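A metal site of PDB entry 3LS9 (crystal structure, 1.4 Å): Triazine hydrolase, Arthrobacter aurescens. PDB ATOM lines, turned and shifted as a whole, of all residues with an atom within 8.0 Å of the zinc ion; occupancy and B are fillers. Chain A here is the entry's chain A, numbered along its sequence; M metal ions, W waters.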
ATOM      1  N   HIS A  63     -17.444 -18.383   2.185  1.00  0.00           N
ATOM      2  CA  HIS A  63     -16.657 -18.308   3.429  1.00  0.00           C
ATOM      3  C   HIS A  63     -17.022 -19.442   4.395  1.00  0.00           C
ATOM      4  O   HIS A  63     -18.079 -19.416   5.006  1.00  0.00           O
ATOM      5  CB  HIS A  63     -16.885 -16.943   4.086  1.00  0.00           C
ATOM      6  CG  HIS A  63     -16.003 -16.683   5.263  1.00  0.00           C
ATOM      7  ND1 HIS A  63     -14.704 -16.215   5.129  1.00  0.00           N
ATOM      8  CD2 HIS A  63     -16.237 -16.775   6.594  1.00  0.00           C
ATOM      9  CE1 HIS A  63     -14.176 -16.057   6.335  1.00  0.00           C
ATOM     10  NE2 HIS A  63     -15.081 -16.377   7.241  1.00  0.00           N
ATOM     11  N   GLN A  64     -16.133 -20.435   4.493  1.00  0.00           N
ATOM     12  CA  GLN A  64     -16.251 -21.546   5.432  1.00  0.00           C
ATOM     13  C   GLN A  64     -15.005 -21.621   6.321  1.00  0.00           C
ATOM     14  O   GLN A  64     -13.962 -21.049   5.998  1.00  0.00           O
ATOM     15  CB  GLN A  64     -16.378 -22.878   4.668  1.00  0.00           C
ATOM     16  CG  GLN A  64     -17.772 -23.473   4.608  1.00  0.00           C
ATOM     17  CD  GLN A  64     -18.257 -24.031   5.934  1.00  0.00           C
ATOM     18  OE1 GLN A  64     -17.579 -23.951   6.961  1.00  0.00           O
ATOM     19  NE2 GLN A  64     -19.463 -24.573   5.914  1.00  0.00           N
ATOM     20  N   HIS A  65     -15.152 -22.316   7.440  1.00  0.00           N
ATOM     21  CA  HIS A  65     -14.009 -22.789   8.236  1.00  0.00           C
ATOM     22  C   HIS A  65     -14.323 -24.254   8.537  1.00  0.00           C
ATOM     23  O   HIS A  65     -14.949 -24.568   9.550  1.00  0.00           O
ATOM     24  CB  HIS A  65     -13.824 -22.005   9.554  1.00  0.00           C
ATOM     25  CG  HIS A  65     -13.671 -20.520   9.368  1.00  0.00           C
ATOM     26  ND1 HIS A  65     -12.628 -19.950   8.666  1.00  0.00           N
ATOM     27  CD2 HIS A  65     -14.416 -19.493   9.822  1.00  0.00           C
ATOM     28  CE1 HIS A  65     -12.754 -18.636   8.680  1.00  0.00           C
ATOM     29  NE2 HIS A  65     -13.834 -18.324   9.371  1.00  0.00           N
ATOM     30  N   GLU A  68     -14.129 -26.498  11.852  1.00  0.00           N
ATOM     31  CA  GLU A  68     -15.077 -26.211  12.930  1.00  0.00           C
ATOM     32  C   GLU A  68     -16.279 -27.144  12.956  1.00  0.00           C
ATOM     33  O   GLU A  68     -17.075 -27.111  13.882  1.00  0.00           O
ATOM     34  CB  GLU A  68     -15.541 -24.770  12.871  1.00  0.00           C
ATOM     35  CG  GLU A  68     -14.442 -23.766  13.181  1.00  0.00           C
ATOM     36  CD  GLU A  68     -14.927 -22.346  13.072  1.00  0.00           C
ATOM     37  OE1 GLU A  68     -16.157 -22.154  13.027  1.00  0.00           O
ATOM     38  OE2 GLU A  68     -14.082 -21.422  13.037  1.00  0.00           O
ATOM     39  N   MET A  82     -17.353 -12.565  21.052  1.00  0.00           N
ATOM     40  CA  MET A  82     -16.241 -12.986  20.203  1.00  0.00           C
ATOM     41  C   MET A  82     -14.961 -13.349  20.944  1.00  0.00           C
ATOM     42  O   MET A  82     -14.353 -14.372  20.662  1.00  0.00           O
ATOM     43  CB  MET A  82     -15.943 -11.930  19.129  1.00  0.00           C
ATOM     44  CG  MET A  82     -14.857 -12.341  18.135  1.00  0.00           C
ATOM     45  SD  MET A  82     -15.303 -13.847  17.258  1.00  0.00           S
ATOM     46  CE  MET A  82     -14.040 -13.887  16.000  1.00  0.00           C
ATOM     47  N   TRP A  85     -15.409 -16.655  22.539  1.00  0.00           N
ATOM     48  CA  TRP A  85     -15.560 -17.645  21.493  1.00  0.00           C
ATOM     49  C   TRP A  85     -14.214 -18.017  20.889  1.00  0.00           C
ATOM     50  O   TRP A  85     -13.889 -19.200  20.758  1.00  0.00           O
ATOM     51  CB  TRP A  85     -16.479 -17.093  20.414  1.00  0.00           C
ATOM     52  CG  TRP A  85     -16.789 -18.061  19.322  1.00  0.00           C
ATOM     53  CD1 TRP A  85     -17.814 -18.970  19.283  1.00  0.00           C
ATOM     54  CD2 TRP A  85     -16.075 -18.217  18.089  1.00  0.00           C
ATOM     55  NE1 TRP A  85     -17.777 -19.679  18.103  1.00  0.00           N
ATOM     56  CE2 TRP A  85     -16.724 -19.234  17.358  1.00  0.00           C
ATOM     57  CE3 TRP A  85     -14.955 -17.587  17.536  1.00  0.00           C
ATOM     58  CZ2 TRP A  85     -16.279 -19.649  16.097  1.00  0.00           C
ATOM     59  CZ3 TRP A  85     -14.518 -17.995  16.285  1.00  0.00           C
ATOM     60  CH2 TRP A  85     -15.183 -19.021  15.579  1.00  0.00           C
ATOM     61  N   GLN A 129     -11.455 -21.247   4.600  1.00  0.00           N
ATOM     62  CA  GLN A 129     -10.336 -20.467   5.126  1.00  0.00           C
ATOM     63  C   GLN A 129      -9.822 -21.183   6.364  1.00  0.00           C
ATOM     64  O   GLN A 129     -10.448 -21.156   7.421  1.00  0.00           O
ATOM     65  CB  GLN A 129     -10.808 -19.035   5.446  1.00  0.00           C
ATOM     66  CG  GLN A 129      -9.670 -18.111   5.911  1.00  0.00           C
ATOM     67  CD  GLN A 129     -10.157 -16.722   6.282  1.00  0.00           C
ATOM     68  OE1 GLN A 129     -11.284 -16.562   6.750  1.00  0.00           O
ATOM     69  NE2 GLN A 129      -9.328 -15.712   6.074  1.00  0.00           N
ATOM     70  N   LEU A 131      -6.911 -21.730   9.166  1.00  0.00           N
ATOM     71  CA  LEU A 131      -5.778 -21.077   9.833  1.00  0.00           C
ATOM     72  C   LEU A 131      -5.019 -21.958  10.819  1.00  0.00           C
ATOM     73  O   LEU A 131      -4.012 -21.529  11.372  1.00  0.00           O
ATOM     74  CB  LEU A 131      -6.199 -19.765  10.524  1.00  0.00           C
ATOM     75  CG  LEU A 131      -7.188 -19.817  11.688  1.00  0.00           C
ATOM     76  CD1 LEU A 131      -6.578 -20.422  12.952  1.00  0.00           C
ATOM     77  CD2 LEU A 131      -7.727 -18.409  12.000  1.00  0.00           C
ATOM     78  N   SER A 161      -5.026 -19.589   5.566  1.00  0.00           N
ATOM     79  CA  SER A 161      -5.136 -18.535   6.567  1.00  0.00           C
ATOM     80  C   SER A 161      -4.080 -18.677   7.654  1.00  0.00           C
ATOM     81  O   SER A 161      -3.294 -19.619   7.656  1.00  0.00           O
ATOM     82  CB  SER A 161      -6.546 -18.548   7.164  1.00  0.00           C
ATOM     83  OG  SER A 161      -6.792 -17.400   7.974  1.00  0.00           O
ATOM     84  N   CYS A 211      -6.203 -14.108   8.552  1.00  0.00           N
ATOM     85  CA  CYS A 211      -7.385 -13.999   9.378  1.00  0.00           C
ATOM     86  C   CYS A 211      -7.892 -12.551   9.463  1.00  0.00           C
ATOM     87  O   CYS A 211      -9.100 -12.312   9.379  1.00  0.00           O
ATOM     88  CB  CYS A 211      -7.121 -14.585  10.769  1.00  0.00           C
ATOM     89  SG  CYS A 211      -8.630 -14.805  11.716  1.00  0.00           S
ATOM     90  N   HIS A 236      -8.276 -12.825   0.468  1.00  0.00           N
ATOM     91  CA  HIS A 236      -9.471 -12.903   1.300  1.00  0.00           C
ATOM     92  C   HIS A 236      -9.120 -12.606   2.754  1.00  0.00           C
ATOM     93  O   HIS A 236      -8.087 -13.072   3.249  1.00  0.00           O
ATOM     94  CB  HIS A 236     -10.062 -14.310   1.189  1.00  0.00           C
ATOM     95  CG  HIS A 236     -11.350 -14.504   1.930  1.00  0.00           C
ATOM     96  ND1 HIS A 236     -12.409 -13.623   1.845  1.00  0.00           N
ATOM     97  CD2 HIS A 236     -11.756 -15.503   2.741  1.00  0.00           C
ATOM     98  CE1 HIS A 236     -13.406 -14.075   2.594  1.00  0.00           C
ATOM     99  NE2 HIS A 236     -13.036 -15.223   3.136  1.00  0.00           N
ATOM    100  N   THR A 237      -9.959 -11.857   3.444  1.00  0.00           N
ATOM    101  CA  THR A 237      -9.784 -11.681   4.883  1.00  0.00           C
ATOM    102  C   THR A 237     -11.093 -11.267   5.532  1.00  0.00           C
ATOM    103  O   THR A 237     -12.065 -10.944   4.821  1.00  0.00           O
ATOM    104  CB  THR A 237      -8.643 -10.672   5.200  1.00  0.00           C
ATOM    105  OG1 THR A 237      -8.258 -10.813   6.574  1.00  0.00           O
ATOM    106  CG2 THR A 237      -9.058  -9.224   4.909  1.00  0.00           C
ATOM    107  N   HIS A 238     -11.136 -11.316   6.854  1.00  0.00           N
ATOM    108  CA  HIS A 238     -12.262 -10.803   7.617  1.00  0.00           C
ATOM    109  C   HIS A 238     -12.187  -9.271   7.643  1.00  0.00           C
ATOM    110  O   HIS A 238     -11.097  -8.697   7.509  1.00  0.00           O
ATOM    111  CB  HIS A 238     -12.240 -11.356   9.058  1.00  0.00           C
ATOM    112  CG  HIS A 238     -12.431 -12.840   9.148  1.00  0.00           C
ATOM    113  ND1 HIS A 238     -11.384 -13.720   9.333  1.00  0.00           N
ATOM    114  CD2 HIS A 238     -13.554 -13.598   9.132  1.00  0.00           C
ATOM    115  CE1 HIS A 238     -11.846 -14.955   9.407  1.00  0.00           C
ATOM    116  NE2 HIS A 238     -13.159 -14.912   9.291  1.00  0.00           N
ATOM    117  N   GLU A 241     -15.432  -6.482  11.576  1.00  0.00           N
ATOM    118  CA  GLU A 241     -16.118  -7.018  12.737  1.00  0.00           C
ATOM    119  C   GLU A 241     -16.052  -5.938  13.820  1.00  0.00           C
ATOM    120  O   GLU A 241     -15.127  -5.117  13.805  1.00  0.00           O
ATOM    121  CB  GLU A 241     -15.433  -8.314  13.203  1.00  0.00           C
ATOM    122  CG  GLU A 241     -15.320  -9.339  12.084  1.00  0.00           C
ATOM    123  CD  GLU A 241     -14.700 -10.649  12.546  1.00  0.00           C
ATOM    124  OE1 GLU A 241     -14.252 -10.718  13.710  1.00  0.00           O
ATOM    125  OE2 GLU A 241     -14.688 -11.591  11.736  1.00  0.00           O
ATOM    126  N   ALA A 273     -14.882 -10.770   4.198  1.00  0.00           N
ATOM    127  CA  ALA A 273     -15.932 -11.428   4.978  1.00  0.00           C
ATOM    128  C   ALA A 273     -16.533 -10.525   6.050  1.00  0.00           C
ATOM    129  O   ALA A 273     -15.803  -9.819   6.751  1.00  0.00           O
ATOM    130  CB  ALA A 273     -15.390 -12.707   5.613  1.00  0.00           C
ATOM    131  N   HIS A 274     -17.858 -10.590   6.164  1.00  0.00           N
ATOM    132  CA  HIS A 274     -18.656  -9.888   7.185  1.00  0.00           C
ATOM    133  C   HIS A 274     -18.952  -8.425   6.836  1.00  0.00           C
ATOM    134  O   HIS A 274     -20.078  -8.083   6.495  1.00  0.00           O
ATOM    135  CB  HIS A 274     -18.047  -9.987   8.592  1.00  0.00           C
ATOM    136  CG  HIS A 274     -17.896 -11.388   9.107  1.00  0.00           C
ATOM    137  ND1 HIS A 274     -18.940 -12.102   9.663  1.00  0.00           N
ATOM    138  CD2 HIS A 274     -16.814 -12.190   9.181  1.00  0.00           C
ATOM    139  CE1 HIS A 274     -18.508 -13.294  10.039  1.00  0.00           C
ATOM    140  NE2 HIS A 274     -17.226 -13.377   9.743  1.00  0.00           N
ATOM    141  N   LEU A 296     -22.426 -12.600   5.771  1.00  0.00           N
ATOM    142  CA  LEU A 296     -22.470 -13.784   6.634  1.00  0.00           C
ATOM    143  C   LEU A 296     -23.462 -13.551   7.770  1.00  0.00           C
ATOM    144  O   LEU A 296     -23.079 -13.312   8.918  1.00  0.00           O
ATOM    145  CB  LEU A 296     -21.065 -14.074   7.179  1.00  0.00           C
ATOM    146  CG  LEU A 296     -19.943 -14.118   6.136  1.00  0.00           C
ATOM    147  CD1 LEU A 296     -18.595 -14.220   6.816  1.00  0.00           C
ATOM    148  CD2 LEU A 296     -20.142 -15.258   5.145  1.00  0.00           C
ATOM    149  N   PRO A 299     -23.383 -15.822  11.554  1.00  0.00           N
ATOM    150  CA  PRO A 299     -22.453 -15.437  12.635  1.00  0.00           C
ATOM    151  C   PRO A 299     -22.615 -13.979  13.060  1.00  0.00           C
ATOM    152  O   PRO A 299     -22.409 -13.665  14.221  1.00  0.00           O
ATOM    153  CB  PRO A 299     -21.061 -15.669  12.002  1.00  0.00           C
ATOM    154  CG  PRO A 299     -21.308 -15.544  10.535  1.00  0.00           C
ATOM    155  CD  PRO A 299     -22.650 -16.190  10.328  1.00  0.00           C
ATOM    156  N   TRP A 305     -23.331  -9.104  16.678  1.00  0.00           N
ATOM    157  CA  TRP A 305     -22.739  -8.003  15.922  1.00  0.00           C
ATOM    158  C   TRP A 305     -23.774  -7.156  15.201  1.00  0.00           C
ATOM    159  O   TRP A 305     -23.618  -5.943  15.063  1.00  0.00           O
ATOM    160  CB  TRP A 305     -21.737  -8.536  14.900  1.00  0.00           C
ATOM    161  CG  TRP A 305     -20.522  -9.164  15.508  1.00  0.00           C
ATOM    162  CD1 TRP A 305     -20.097  -9.055  16.798  1.00  0.00           C
ATOM    163  CD2 TRP A 305     -19.571  -9.985  14.837  1.00  0.00           C
ATOM    164  NE1 TRP A 305     -18.932  -9.775  16.970  1.00  0.00           N
ATOM    165  CE2 TRP A 305     -18.587 -10.343  15.781  1.00  0.00           C
ATOM    166  CE3 TRP A 305     -19.448 -10.445  13.517  1.00  0.00           C
ATOM    167  CZ2 TRP A 305     -17.512 -11.157  15.450  1.00  0.00           C
ATOM    168  CZ3 TRP A 305     -18.372 -11.250  13.190  1.00  0.00           C
ATOM    169  CH2 TRP A 305     -17.410 -11.596  14.159  1.00  0.00           C
ATOM    170  N   THR A 324     -21.629 -19.002   4.964  1.00  0.00           N
ATOM    171  CA  THR A 324     -22.120 -19.500   6.253  1.00  0.00           C
ATOM    172  C   THR A 324     -21.174 -19.254   7.423  1.00  0.00           C
ATOM    173  O   THR A 324     -21.596 -19.264   8.577  1.00  0.00           O
ATOM    174  CB  THR A 324     -22.420 -21.007   6.214  1.00  0.00           C
ATOM    175  OG1 THR A 324     -21.221 -21.731   5.902  1.00  0.00           O
ATOM    176  CG2 THR A 324     -23.458 -21.320   5.168  1.00  0.00           C
ATOM    177  N   THR A 325     -19.895 -19.048   7.116  1.00  0.00           N
ATOM    178  CA  THR A 325     -18.778 -19.240   8.051  1.00  0.00           C
ATOM    179  C   THR A 325     -18.739 -20.662   8.613  1.00  0.00           C
ATOM    180  O   THR A 325     -19.468 -21.557   8.149  1.00  0.00           O
ATOM    181  CB  THR A 325     -18.654 -18.147   9.145  1.00  0.00           C
ATOM    182  OG1 THR A 325     -17.282 -18.099   9.544  1.00  0.00           O
ATOM    183  CG2 THR A 325     -19.504 -18.456  10.369  1.00  0.00           C
ATOM    184  N   GLY A 326     -17.848 -20.886   9.566  1.00  0.00           N
ATOM    185  CA  GLY A 326     -17.654 -22.201  10.128  1.00  0.00           C
ATOM    186  C   GLY A 326     -18.717 -22.619  11.115  1.00  0.00           C
ATOM    187  O   GLY A 326     -19.442 -21.803  11.675  1.00  0.00           O
ATOM    188  N   SER A 329     -19.689 -21.264  14.749  1.00  0.00           N
ATOM    189  CA  SER A 329     -20.460 -20.041  14.905  1.00  0.00           C
ATOM    190  C   SER A 329     -21.531 -19.957  13.830  1.00  0.00           C
ATOM    191  O   SER A 329     -21.608 -18.974  13.079  1.00  0.00           O
ATOM    192  CB  SER A 329     -19.578 -18.801  14.837  1.00  0.00           C
ATOM    193  OG  SER A 329     -19.006 -18.661  13.553  1.00  0.00           O
HETATM  194 ZN    ZN M   1     -14.506 -16.430   9.211  1.00  0.00          ZN
HETATM  195  O   HOH W   1     -16.069 -15.719  10.288  1.00  0.00           O
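A ring nitrogen (ND1) of His 65 is in hydrogen-bond range of the backbone carbonyl oxygen (O) of Gln 129 (2.8 Å). A ring nitrogen (NE2) of His 236 sits at hydrogen-bond distance from a ring nitrogen (ND1) of His 63 (2.8 Å). The backbone carbonyl oxygen (O) of His 63 lies within hydrogen-bond range of the backbone NH (N) of Thr 325. OG1 of Thr 325 lies close to NE2 of His 65 (3.5 Å). The backbone carbonyl oxygen (O) of Thr 325 sits close to the side-chain amide oxygen (OE1) of Gln 64 (3.3 Å). ND1 of His 238 lies within hydrogen-bond range of O of Cys 211 (2.7 Å).
The zinc ion is bound by NE2 of His 65. The zinc ion is bound by water W1 (2.0 Å). NE2 of His 238 is bound to the zinc ion (2.0 Å). The zinc ion is bound by a ring nitrogen (NE2) of His 63, 2.1 Å away.
Merely in contact with the zinc ion: Thr 325 (3.3 Å). Four residues have an atom within 4 Å of the zinc ion: His 63, His 65, His 238 and Thr 325.
Water W1 lies within hydrogen-bond range of a ring nitrogen (NE2) of His 274 (2.7 Å) and the side-chain hydroxyl of Thr 325 (2.8 Å).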
